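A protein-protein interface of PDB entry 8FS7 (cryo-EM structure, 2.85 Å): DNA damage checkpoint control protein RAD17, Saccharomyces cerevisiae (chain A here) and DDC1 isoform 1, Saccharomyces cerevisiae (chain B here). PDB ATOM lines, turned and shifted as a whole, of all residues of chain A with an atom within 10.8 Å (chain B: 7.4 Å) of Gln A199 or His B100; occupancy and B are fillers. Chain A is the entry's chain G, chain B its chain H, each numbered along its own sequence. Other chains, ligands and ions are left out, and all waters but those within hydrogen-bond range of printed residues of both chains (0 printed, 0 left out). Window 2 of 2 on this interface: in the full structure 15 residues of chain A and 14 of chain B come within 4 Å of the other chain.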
ATOM      1  N   ASP A 169      36.017  -6.361   9.572  1.00  0.00           N
ATOM      2  CA  ASP A 169      34.569  -6.172   9.542  1.00  0.00           C
ATOM      3  C   ASP A 169      33.972  -6.685   8.237  1.00  0.00           C
ATOM      4  O   ASP A 169      32.876  -7.258   8.233  1.00  0.00           O
ATOM      5  CB  ASP A 169      34.214  -4.701   9.746  1.00  0.00           C
ATOM      6  CG  ASP A 169      32.754  -4.505  10.103  1.00  0.00           C
ATOM      7  OD1 ASP A 169      32.097  -5.496  10.488  1.00  0.00           O
ATOM      8  OD2 ASP A 169      32.255  -3.368   9.987  1.00  0.00           O
ATOM      9  N   LEU A 170      34.669  -6.477   7.117  1.00  0.00           N
ATOM     10  CA  LEU A 170      34.205  -7.032   5.848  1.00  0.00           C
ATOM     11  C   LEU A 170      34.186  -8.555   5.890  1.00  0.00           C
ATOM     12  O   LEU A 170      33.245  -9.186   5.397  1.00  0.00           O
ATOM     13  CB  LEU A 170      35.087  -6.537   4.702  1.00  0.00           C
ATOM     14  CG  LEU A 170      34.878  -5.096   4.231  1.00  0.00           C
ATOM     15  CD1 LEU A 170      35.550  -4.870   2.884  1.00  0.00           C
ATOM     16  CD2 LEU A 170      33.398  -4.753   4.157  1.00  0.00           C
ATOM     17  N   LYS A 171      35.217  -9.162   6.483  1.00  0.00           N
ATOM     18  CA  LYS A 171      35.261 -10.616   6.599  1.00  0.00           C
ATOM     19  C   LYS A 171      34.123 -11.138   7.469  1.00  0.00           C
ATOM     20  O   LYS A 171      33.529 -12.180   7.170  1.00  0.00           O
ATOM     21  CB  LYS A 171      36.614 -11.052   7.162  1.00  0.00           C
ATOM     22  CG  LYS A 171      36.742 -12.548   7.407  1.00  0.00           C
ATOM     23  CD  LYS A 171      36.675 -13.330   6.107  1.00  0.00           C
ATOM     24  CE  LYS A 171      36.843 -14.821   6.352  1.00  0.00           C
ATOM     25  NZ  LYS A 171      36.770 -15.603   5.087  1.00  0.00           N
ATOM     26  N   GLU A 172      33.800 -10.422   8.547  1.00  0.00           N
ATOM     27  CA  GLU A 172      32.775 -10.876   9.481  1.00  0.00           C
ATOM     28  C   GLU A 172      31.358 -10.755   8.932  1.00  0.00           C
ATOM     29  O   GLU A 172      30.434 -11.309   9.537  1.00  0.00           O
ATOM     30  CB  GLU A 172      32.886 -10.097  10.793  1.00  0.00           C
ATOM     31  CG  GLU A 172      33.592 -10.857  11.905  1.00  0.00           C
ATOM     32  CD  GLU A 172      34.579  -9.994  12.665  1.00  0.00           C
ATOM     33  OE1 GLU A 172      34.337  -8.775  12.784  1.00  0.00           O
ATOM     34  OE2 GLU A 172      35.599 -10.534  13.142  1.00  0.00           O
ATOM     35  N   ILE A 173      31.160 -10.059   7.816  1.00  0.00           N
ATOM     36  CA  ILE A 173      29.837  -9.888   7.227  1.00  0.00           C
ATOM     37  C   ILE A 173      29.710 -10.653   5.910  1.00  0.00           C
ATOM     38  O   ILE A 173      28.818 -10.372   5.111  1.00  0.00           O
ATOM     39  CB  ILE A 173      29.493  -8.398   7.057  1.00  0.00           C
ATOM     40  CG1 ILE A 173      30.402  -7.735   6.015  1.00  0.00           C
ATOM     41  CG2 ILE A 173      29.583  -7.673   8.391  1.00  0.00           C
ATOM     42  CD1 ILE A 173      29.690  -7.311   4.747  1.00  0.00           C
ATOM     43  N   GLY A 174      30.570 -11.643   5.688  1.00  0.00           N
ATOM     44  CA  GLY A 174      30.559 -12.406   4.455  1.00  0.00           C
ATOM     45  C   GLY A 174      31.369 -11.759   3.352  1.00  0.00           C
ATOM     46  O   GLY A 174      32.492 -12.193   3.074  1.00  0.00           O
ATOM     47  N   CYS A 175      30.816 -10.715   2.728  1.00  0.00           N
ATOM     48  CA  CYS A 175      31.503  -9.919   1.709  1.00  0.00           C
ATOM     49  C   CYS A 175      32.002 -10.803   0.560  1.00  0.00           C
ATOM     50  O   CYS A 175      33.195 -11.043   0.392  1.00  0.00           O
ATOM     51  CB  CYS A 175      32.654  -9.114   2.324  1.00  0.00           C
ATOM     52  SG  CYS A 175      33.492  -7.995   1.178  1.00  0.00           S
ATOM     53  N   LYS A 176      31.039 -11.330  -0.199  1.00  0.00           N
ATOM     54  CA  LYS A 176      31.396 -12.104  -1.384  1.00  0.00           C
ATOM     55  C   LYS A 176      32.155 -11.258  -2.400  1.00  0.00           C
ATOM     56  O   LYS A 176      33.067 -11.761  -3.067  1.00  0.00           O
ATOM     57  CB  LYS A 176      30.144 -12.710  -2.018  1.00  0.00           C
ATOM     58  CG  LYS A 176      29.549 -13.856  -1.218  1.00  0.00           C
ATOM     59  CD  LYS A 176      30.568 -14.965  -1.011  1.00  0.00           C
ATOM     60  CE  LYS A 176      30.550 -15.472   0.422  1.00  0.00           C
ATOM     61  NZ  LYS A 176      31.836 -16.120   0.802  1.00  0.00           N
ATOM     62  N   GLU A 177      31.802  -9.981  -2.530  1.00  0.00           N
ATOM     63  CA  GLU A 177      32.489  -9.059  -3.424  1.00  0.00           C
ATOM     64  C   GLU A 177      32.737  -7.742  -2.701  1.00  0.00           C
ATOM     65  O   GLU A 177      32.035  -7.390  -1.751  1.00  0.00           O
ATOM     66  CB  GLU A 177      31.687  -8.814  -4.710  1.00  0.00           C
ATOM     67  CG  GLU A 177      31.489 -10.052  -5.568  1.00  0.00           C
ATOM     68  CD  GLU A 177      30.342  -9.905  -6.548  1.00  0.00           C
ATOM     69  OE1 GLU A 177      29.517  -8.985  -6.366  1.00  0.00           O
ATOM     70  OE2 GLU A 177      30.265 -10.710  -7.499  1.00  0.00           O
ATOM     71  N   CYS A 178      33.753  -7.013  -3.163  1.00  0.00           N
ATOM     72  CA  CYS A 178      34.151  -5.759  -2.540  1.00  0.00           C
ATOM     73  C   CYS A 178      34.395  -4.703  -3.610  1.00  0.00           C
ATOM     74  O   CYS A 178      34.705  -5.021  -4.761  1.00  0.00           O
ATOM     75  CB  CYS A 178      35.411  -5.933  -1.681  1.00  0.00           C
ATOM     76  SG  CYS A 178      35.979  -4.419  -0.872  1.00  0.00           S
ATOM     77  N   SER A 196      30.782  -3.237  -0.261  1.00  0.00           N
ATOM     78  CA  SER A 196      30.847  -4.690  -0.294  1.00  0.00           C
ATOM     79  C   SER A 196      29.511  -5.291  -0.708  1.00  0.00           C
ATOM     80  O   SER A 196      28.447  -4.796  -0.325  1.00  0.00           O
ATOM     81  CB  SER A 196      31.266  -5.250   1.070  1.00  0.00           C
ATOM     82  OG  SER A 196      30.145  -5.690   1.814  1.00  0.00           O
ATOM     83  N   LYS A 197      29.585  -6.361  -1.497  1.00  0.00           N
ATOM     84  CA  LYS A 197      28.448  -7.219  -1.808  1.00  0.00           C
ATOM     85  C   LYS A 197      28.466  -8.425  -0.878  1.00  0.00           C
ATOM     86  O   LYS A 197      29.471  -9.139  -0.802  1.00  0.00           O
ATOM     87  CB  LYS A 197      28.485  -7.669  -3.270  1.00  0.00           C
ATOM     88  CG  LYS A 197      27.124  -7.872  -3.951  1.00  0.00           C
ATOM     89  CD  LYS A 197      25.993  -6.982  -3.444  1.00  0.00           C
ATOM     90  CE  LYS A 197      26.164  -5.517  -3.819  1.00  0.00           C
ATOM     91  NZ  LYS A 197      24.888  -4.784  -3.601  1.00  0.00           N
ATOM     92  N   SER A 198      27.358  -8.649  -0.177  1.00  0.00           N
ATOM     93  CA  SER A 198      27.265  -9.737   0.784  1.00  0.00           C
ATOM     94  C   SER A 198      25.805 -10.148   0.930  1.00  0.00           C
ATOM     95  O   SER A 198      24.931  -9.699   0.183  1.00  0.00           O
ATOM     96  CB  SER A 198      27.863  -9.332   2.134  1.00  0.00           C
ATOM     97  OG  SER A 198      27.296  -8.123   2.609  1.00  0.00           O
ATOM     98  N   GLN A 199      25.551 -11.026   1.903  1.00  0.00           N
ATOM     99  CA  GLN A 199      24.180 -11.418   2.208  1.00  0.00           C
ATOM    100  C   GLN A 199      23.372 -10.243   2.741  1.00  0.00           C
ATOM    101  O   GLN A 199      22.152 -10.193   2.555  1.00  0.00           O
ATOM    102  CB  GLN A 199      24.179 -12.569   3.212  1.00  0.00           C
ATOM    103  CG  GLN A 199      25.177 -12.397   4.344  1.00  0.00           C
ATOM    104  CD  GLN A 199      25.224 -13.597   5.268  1.00  0.00           C
ATOM    105  OE1 GLN A 199      24.478 -14.560   5.092  1.00  0.00           O
ATOM    106  NE2 GLN A 199      26.106 -13.546   6.258  1.00  0.00           N
ATOM    107  N   LEU A 200      24.035  -9.294   3.409  1.00  0.00           N
ATOM    108  CA  LEU A 200      23.339  -8.114   3.910  1.00  0.00           C
ATOM    109  C   LEU A 200      22.856  -7.219   2.779  1.00  0.00           C
ATOM    110  O   LEU A 200      21.805  -6.578   2.899  1.00  0.00           O
ATOM    111  CB  LEU A 200      24.250  -7.330   4.855  1.00  0.00           C
ATOM    112  CG  LEU A 200      24.275  -7.806   6.307  1.00  0.00           C
ATOM    113  CD1 LEU A 200      25.623  -7.526   6.946  1.00  0.00           C
ATOM    114  CD2 LEU A 200      23.163  -7.137   7.096  1.00  0.00           C
ATOM    115  N   GLY A 201      23.595  -7.163   1.676  1.00  0.00           N
ATOM    116  CA  GLY A 201      23.247  -6.276   0.585  1.00  0.00           C
ATOM    117  C   GLY A 201      24.356  -5.298   0.265  1.00  0.00           C
ATOM    118  O   GLY A 201      25.438  -5.698  -0.175  1.00  0.00           O
ATOM    119  N   PHE A 202      24.095  -4.012   0.480  1.00  0.00           N
ATOM    120  CA  PHE A 202      25.081  -2.959   0.275  1.00  0.00           C
ATOM    121  C   PHE A 202      25.688  -2.593   1.621  1.00  0.00           C
ATOM    122  O   PHE A 202      24.977  -2.155   2.532  1.00  0.00           O
ATOM    123  CB  PHE A 202      24.455  -1.732  -0.387  1.00  0.00           C
ATOM    124  CG  PHE A 202      24.692  -1.654  -1.869  1.00  0.00           C
ATOM    125  CD1 PHE A 202      25.924  -1.995  -2.399  1.00  0.00           C
ATOM    126  CD2 PHE A 202      23.690  -1.234  -2.734  1.00  0.00           C
ATOM    127  CE1 PHE A 202      26.156  -1.926  -3.761  1.00  0.00           C
ATOM    128  CE2 PHE A 202      23.915  -1.163  -4.098  1.00  0.00           C
ATOM    129  CZ  PHE A 202      25.150  -1.511  -4.611  1.00  0.00           C
ATOM    130  N   SER A 203      26.995  -2.783   1.739  1.00  0.00           N
ATOM    131  CA  SER A 203      27.752  -2.466   2.939  1.00  0.00           C
ATOM    132  C   SER A 203      28.913  -1.561   2.574  1.00  0.00           C
ATOM    133  O   SER A 203      29.666  -1.867   1.649  1.00  0.00           O
ATOM    134  CB  SER A 203      28.295  -3.730   3.594  1.00  0.00           C
ATOM    135  OG  SER A 203      28.392  -3.567   4.987  1.00  0.00           O
ATOM    136  N   PHE A 239      36.787 -10.671  -2.954  1.00  0.00           N
ATOM    137  CA  PHE A 239      37.226 -10.561  -1.567  1.00  0.00           C
ATOM    138  C   PHE A 239      38.097 -11.730  -1.129  1.00  0.00           C
ATOM    139  O   PHE A 239      38.780 -11.623  -0.106  1.00  0.00           O
ATOM    140  CB  PHE A 239      36.017 -10.435  -0.644  1.00  0.00           C
ATOM    141  CG  PHE A 239      36.369 -10.093   0.777  1.00  0.00           C
ATOM    142  CD1 PHE A 239      36.878  -8.846   1.098  1.00  0.00           C
ATOM    143  CD2 PHE A 239      36.191 -11.021   1.790  1.00  0.00           C
ATOM    144  CE1 PHE A 239      37.202  -8.530   2.404  1.00  0.00           C
ATOM    145  CE2 PHE A 239      36.514 -10.711   3.097  1.00  0.00           C
ATOM    146  CZ  PHE A 239      37.020  -9.464   3.405  1.00  0.00           C
ATOM    147  N   ILE B  20      19.943  -8.889  20.942  1.00  0.00           N
ATOM    148  CA  ILE B  20      19.776  -9.230  19.531  1.00  0.00           C
ATOM    149  C   ILE B  20      20.296 -10.637  19.255  1.00  0.00           C
ATOM    150  O   ILE B  20      19.659 -11.422  18.540  1.00  0.00           O
ATOM    151  CB  ILE B  20      20.468  -8.180  18.641  1.00  0.00           C
ATOM    152  CG1 ILE B  20      19.719  -6.848  18.712  1.00  0.00           C
ATOM    153  CG2 ILE B  20      20.553  -8.660  17.202  1.00  0.00           C
ATOM    154  CD1 ILE B  20      18.254  -6.951  18.349  1.00  0.00           C
ATOM    155  N   SER B  24      18.116 -13.841  18.041  1.00  0.00           N
ATOM    156  CA  SER B  24      18.520 -14.643  16.890  1.00  0.00           C
ATOM    157  C   SER B  24      18.615 -16.122  17.244  1.00  0.00           C
ATOM    158  O   SER B  24      18.241 -16.977  16.433  1.00  0.00           O
ATOM    159  CB  SER B  24      19.854 -14.141  16.340  1.00  0.00           C
ATOM    160  OG  SER B  24      20.914 -14.421  17.237  1.00  0.00           O
ATOM    161  N   ASP B  28      15.273 -17.544  13.626  1.00  0.00           N
ATOM    162  CA  ASP B  28      16.166 -17.017  12.598  1.00  0.00           C
ATOM    163  C   ASP B  28      15.826 -15.588  12.188  1.00  0.00           C
ATOM    164  O   ASP B  28      16.686 -14.901  11.629  1.00  0.00           O
ATOM    165  CB  ASP B  28      16.139 -17.926  11.369  1.00  0.00           C
ATOM    166  CG  ASP B  28      14.811 -17.882  10.640  1.00  0.00           C
ATOM    167  OD1 ASP B  28      13.760 -17.945  11.313  1.00  0.00           O
ATOM    168  OD2 ASP B  28      14.817 -17.786   9.395  1.00  0.00           O
ATOM    169  N   ASP B  29      14.605 -15.126  12.448  1.00  0.00           N
ATOM    170  CA  ASP B  29      14.195 -13.771  12.100  1.00  0.00           C
ATOM    171  C   ASP B  29      13.738 -13.045  13.356  1.00  0.00           C
ATOM    172  O   ASP B  29      12.964 -13.593  14.147  1.00  0.00           O
ATOM    173  CB  ASP B  29      13.076 -13.782  11.052  1.00  0.00           C
ATOM    174  CG  ASP B  29      13.594 -13.548   9.646  1.00  0.00           C
ATOM    175  OD1 ASP B  29      14.702 -14.033   9.332  1.00  0.00           O
ATOM    176  OD2 ASP B  29      12.897 -12.880   8.856  1.00  0.00           O
ATOM    177  N   VAL B  96      13.282  -8.658  10.524  1.00  0.00           N
ATOM    178  CA  VAL B  96      14.669  -8.576  10.088  1.00  0.00           C
ATOM    179  C   VAL B  96      15.371  -9.883  10.437  1.00  0.00           C
ATOM    180  O   VAL B  96      14.953 -10.612  11.342  1.00  0.00           O
ATOM    181  CB  VAL B  96      15.394  -7.362  10.723  1.00  0.00           C
ATOM    182  CG1 VAL B  96      15.754  -7.639  12.176  1.00  0.00           C
ATOM    183  CG2 VAL B  96      16.623  -6.968   9.910  1.00  0.00           C
ATOM    184  N   ASN B  97      16.433 -10.187   9.693  1.00  0.00           N
ATOM    185  CA  ASN B  97      17.186 -11.413   9.921  1.00  0.00           C
ATOM    186  C   ASN B  97      17.983 -11.310  11.216  1.00  0.00           C
ATOM    187  O   ASN B  97      18.669 -10.313  11.459  1.00  0.00           O
ATOM    188  CB  ASN B  97      18.119 -11.686   8.741  1.00  0.00           C
ATOM    189  CG  ASN B  97      18.657 -13.106   8.732  1.00  0.00           C
ATOM    190  OD1 ASN B  97      18.511 -13.848   9.703  1.00  0.00           O
ATOM    191  ND2 ASN B  97      19.284 -13.491   7.629  1.00  0.00           N
ATOM    192  N   GLY B  98      17.886 -12.347  12.050  1.00  0.00           N
ATOM    193  CA  GLY B  98      18.608 -12.341  13.313  1.00  0.00           C
ATOM    194  C   GLY B  98      20.113 -12.404  13.141  1.00  0.00           C
ATOM    195  O   GLY B  98      20.853 -11.672  13.805  1.00  0.00           O
ATOM    196  N   ARG B  99      20.589 -13.282  12.254  1.00  0.00           N
ATOM    197  CA  ARG B  99      22.027 -13.417  12.045  1.00  0.00           C
ATOM    198  C   ARG B  99      22.616 -12.164  11.408  1.00  0.00           C
ATOM    199  O   ARG B  99      23.734 -11.757  11.745  1.00  0.00           O
ATOM    200  CB  ARG B  99      22.320 -14.647  11.186  1.00  0.00           C
ATOM    201  CG  ARG B  99      21.980 -15.966  11.861  1.00  0.00           C
ATOM    202  CD  ARG B  99      22.502 -17.153  11.066  1.00  0.00           C
ATOM    203  NE  ARG B  99      21.706 -17.407   9.872  1.00  0.00           N
ATOM    204  CZ  ARG B  99      22.062 -17.051   8.644  1.00  0.00           C
ATOM    205  NH1 ARG B  99      23.203 -16.423   8.409  1.00  0.00           N
ATOM    206  NH2 ARG B  99      21.253 -17.334   7.627  1.00  0.00           N
ATOM    207  N   HIS B 100      21.883 -11.547  10.479  1.00  0.00           N
ATOM    208  CA  HIS B 100      22.358 -10.312   9.864  1.00  0.00           C
ATOM    209  C   HIS B 100      22.403  -9.170  10.871  1.00  0.00           C
ATOM    210  O   HIS B 100      23.314  -8.336  10.832  1.00  0.00           O
ATOM    211  CB  HIS B 100      21.475  -9.946   8.672  1.00  0.00           C
ATOM    212  CG  HIS B 100      21.621 -10.872   7.505  1.00  0.00           C
ATOM    213  ND1 HIS B 100      20.678 -10.963   6.504  1.00  0.00           N
ATOM    214  CD2 HIS B 100      22.601 -11.748   7.180  1.00  0.00           C
ATOM    215  CE1 HIS B 100      21.071 -11.855   5.612  1.00  0.00           C
ATOM    216  NE2 HIS B 100      22.234 -12.347   6.000  1.00  0.00           N
ATOM    217  N   LEU B 101      21.423  -9.108  11.776  1.00  0.00           N
ATOM    218  CA  LEU B 101      21.399  -8.026  12.755  1.00  0.00           C
ATOM    219  C   LEU B 101      22.440  -8.226  13.849  1.00  0.00           C
ATOM    220  O   LEU B 101      23.012  -7.247  14.341  1.00  0.00           O
ATOM    221  CB  LEU B 101      20.004  -7.898  13.366  1.00  0.00           C
ATOM    222  CG  LEU B 101      19.736  -6.608  14.145  1.00  0.00           C
ATOM    223  CD1 LEU B 101      20.043  -5.390  13.288  1.00  0.00           C
ATOM    224  CD2 LEU B 101      18.302  -6.567  14.645  1.00  0.00           C
ATOM    225  N   THR B 102      22.700  -9.474  14.246  1.00  0.00           N
ATOM    226  CA  THR B 102      23.642  -9.728  15.330  1.00  0.00           C
ATOM    227  C   THR B 102      25.097  -9.588  14.898  1.00  0.00           C
ATOM    228  O   THR B 102      25.972  -9.451  15.760  1.00  0.00           O
ATOM    229  CB  THR B 102      23.411 -11.122  15.922  1.00  0.00           C
ATOM    230  OG1 THR B 102      24.055 -11.211  17.199  1.00  0.00           O
ATOM    231  CG2 THR B 102      23.970 -12.195  15.006  1.00  0.00           C
ATOM    232  N   THR B 103      25.378  -9.622  13.597  1.00  0.00           N
ATOM    233  CA  THR B 103      26.726  -9.393  13.093  1.00  0.00           C
ATOM    234  C   THR B 103      27.000  -7.919  12.828  1.00  0.00           C
ATOM    235  O   THR B 103      28.123  -7.566  12.452  1.00  0.00           O
ATOM    236  CB  THR B 103      26.965 -10.208  11.815  1.00  0.00           C
ATOM    237  OG1 THR B 103      28.373 -10.334  11.582  1.00  0.00           O
ATOM    238  CG2 THR B 103      26.315  -9.536  10.615  1.00  0.00           C
ATOM    239  N   ILE B 104      26.003  -7.060  13.017  1.00  0.00           N
ATOM    240  CA  ILE B 104      26.169  -5.620  12.862  1.00  0.00           C
ATOM    241  C   ILE B 104      26.436  -4.948  14.201  1.00  0.00           C
ATOM    242  O   ILE B 104      27.324  -4.099  14.320  1.00  0.00           O
ATOM    243  CB  ILE B 104      24.918  -5.029  12.175  1.00  0.00           C
ATOM    244  CG1 ILE B 104      24.859  -5.456  10.708  1.00  0.00           C
ATOM    245  CG2 ILE B 104      24.884  -3.519  12.314  1.00  0.00           C
ATOM    246  CD1 ILE B 104      23.643  -4.936   9.979  1.00  0.00           C
ATOM    247  N   SER B 105      25.683  -5.333  15.230  1.00  0.00           N
ATOM    248  CA  SER B 105      25.762  -4.704  16.542  1.00  0.00           C
ATOM    249  C   SER B 105      26.894  -5.250  17.403  1.00  0.00           C
ATOM    250  O   SER B 105      27.040  -4.812  18.548  1.00  0.00           O
ATOM    251  CB  SER B 105      24.431  -4.870  17.279  1.00  0.00           C
ATOM    252  OG  SER B 105      24.051  -6.234  17.340  1.00  0.00           O
ATOM    253  N   VAL B 136      21.267   1.298   9.572  1.00  0.00           N
ATOM    254  CA  VAL B 136      22.025   1.278  10.816  1.00  0.00           C
ATOM    255  C   VAL B 136      23.387   1.900  10.546  1.00  0.00           C
ATOM    256  O   VAL B 136      24.095   1.475   9.629  1.00  0.00           O
ATOM    257  CB  VAL B 136      22.171  -0.148  11.380  1.00  0.00           C
ATOM    258  CG1 VAL B 136      22.373  -1.158  10.256  1.00  0.00           C
ATOM    259  CG2 VAL B 136      23.311  -0.213  12.386  1.00  0.00           C
ATOM    260  N   TYR B 148      25.215  -0.050   7.367  1.00  0.00           N
ATOM    261  CA  TYR B 148      24.686  -1.184   6.626  1.00  0.00           C
ATOM    262  C   TYR B 148      23.246  -0.910   6.213  1.00  0.00           C
ATOM    263  O   TYR B 148      22.584  -0.018   6.751  1.00  0.00           O
ATOM    264  CB  TYR B 148      24.724  -2.473   7.461  1.00  0.00           C
ATOM    265  CG  TYR B 148      26.045  -2.747   8.141  1.00  0.00           C
ATOM    266  CD1 TYR B 148      26.326  -2.215   9.387  1.00  0.00           C
ATOM    267  CD2 TYR B 148      26.997  -3.555   7.549  1.00  0.00           C
ATOM    268  CE1 TYR B 148      27.532  -2.464  10.015  1.00  0.00           C
ATOM    269  CE2 TYR B 148      28.208  -3.808   8.164  1.00  0.00           C
ATOM    270  CZ  TYR B 148      28.468  -3.261   9.398  1.00  0.00           C
ATOM    271  OH  TYR B 148      29.670  -3.519  10.016  1.00  0.00           O
ATOM    272  N   CYS B 149      22.761  -1.701   5.257  1.00  0.00           N
ATOM    273  CA  CYS B 149      21.372  -1.636   4.799  1.00  0.00           C
ATOM    274  C   CYS B 149      20.776  -3.039   4.728  1.00  0.00           C
ATOM    275  O   CYS B 149      20.559  -3.578   3.635  1.00  0.00           O
ATOM    276  CB  CYS B 149      21.284  -0.939   3.440  1.00  0.00           C
ATOM    277  SG  CYS B 149      21.742   0.808   3.466  1.00  0.00           S
ATOM    278  N   PRO B 150      20.499  -3.663   5.874  1.00  0.00           N
ATOM    279  CA  PRO B 150      19.823  -4.966   5.850  1.00  0.00           C
ATOM    280  C   PRO B 150      18.391  -4.850   5.357  1.00  0.00           C
ATOM    281  O   PRO B 150      17.717  -3.836   5.555  1.00  0.00           O
ATOM    282  CB  PRO B 150      19.866  -5.417   7.314  1.00  0.00           C
ATOM    283  CG  PRO B 150      19.988  -4.160   8.090  1.00  0.00           C
ATOM    284  CD  PRO B 150      20.828  -3.249   7.250  1.00  0.00           C
ATOM    285  N   GLN B 151      17.926  -5.916   4.710  1.00  0.00           N
ATOM    286  CA  GLN B 151      16.555  -5.974   4.225  1.00  0.00           C
ATOM    287  C   GLN B 151      15.602  -6.283   5.372  1.00  0.00           C
ATOM    288  O   GLN B 151      15.906  -7.099   6.247  1.00  0.00           O
ATOM    289  CB  GLN B 151      16.420  -7.036   3.136  1.00  0.00           C
ATOM    290  CG  GLN B 151      17.490  -6.967   2.060  1.00  0.00           C
ATOM    291  CD  GLN B 151      16.990  -6.327   0.780  1.00  0.00           C
ATOM    292  OE1 GLN B 151      15.866  -5.831   0.719  1.00  0.00           O
ATOM    293  NE2 GLN B 151      17.826  -6.336  -0.251  1.00  0.00           N
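The side-chain hydroxyl of Thr B103 lies within hydrogen-bond range of the backbone carbonyl oxygen of Glu A172 (3.1 Å). O of Leu A200 sits close to O of Cys B149, 3.3 Å away. OD2 of Asp A169 is in hydrogen-bond range of OH of Tyr B148, at 2.6 Å. OE1 of Gln A199 lies within hydrogen-bond range of NE2 of His B100 (3.3 Å).
The backbone NH of Tyr B148 is in hydrogen-bond range of the backbone carbonyl oxygen of Val B136, 2.9 Å away. ND2 of Asn B97 is in hydrogen-bond range of ND1 of His B100. The backbone NH (N) of Ser A196 sits at hydrogen-bond distance from the backbone carbonyl oxygen (O) of Ser A203 (2.6 Å).
CB of His B100 touches CD2 of Leu A200 (3.6 Å). CD2 of Leu A200 touches CD1 of Ile B104, 3.7 Å away. Pro B150 touches Leu A200. N of Cys B149 touches O of Phe A202, at 3.5 Å. OG of Ser A203 touches CD2 of Tyr B148, at 2.9 Å.
Printed residues of chain B that touch a printed residue of chain A: His B100, Thr B103, Ile B104, Tyr B148, Cys B149 and Pro B150. Hydrophobic or aromatic side chains of chain B within 4 Å of the printed part of chain A: His B100, Ile B104, Tyr B148 and Pro B150. Of the 19 printed residues of chain A, 6 touch a printed residue of chain B. Hydrophobic or aromatic side chains of chain A that line the printed part of chain B: Leu A200. Among the printed residues, no Asp or Glu carboxylate lies within 4 Å of a Lys or Arg side-chain nitrogen of the other chain.
Of the printed residues of chain B, Glu A172 touches Thr B103. Of the printed residues of chain B, Gln A199 touches His B100. Of the printed residues of chain B, Leu A200 touches His B100, Ile B104, Cys B149 and Pro B150. Printed residues of chain B within 4 Å of Phe A202: Cys B149. No residue of chain A comes within 4 Å of Asn B97. No residue of chain A comes within 4 Å of Gly B98. Of the printed residues of chain A, His B100 touches Gln A199 (3.3 Å) and Leu A200 (3.6 Å). Leu B101 touches none of the printed residues of chain A. Of chain A, only Glu A172 (3.1 Å) comes within 4 Å of Thr B103. Of the printed residues of chain A, Cys B149 touches Leu A200 (3.3 Å) and Phe A202 (3.5 Å). Of the printed residues of chain A, Pro B150 touches Leu A200 (3.7 Å). The nearest printed residue of chain B that does not touch Gln A199 is Arg B99 (4.01 Å). The nearest printed residue of chain B that does not touch Glu A172 is Ile B104 (7.1 Å).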
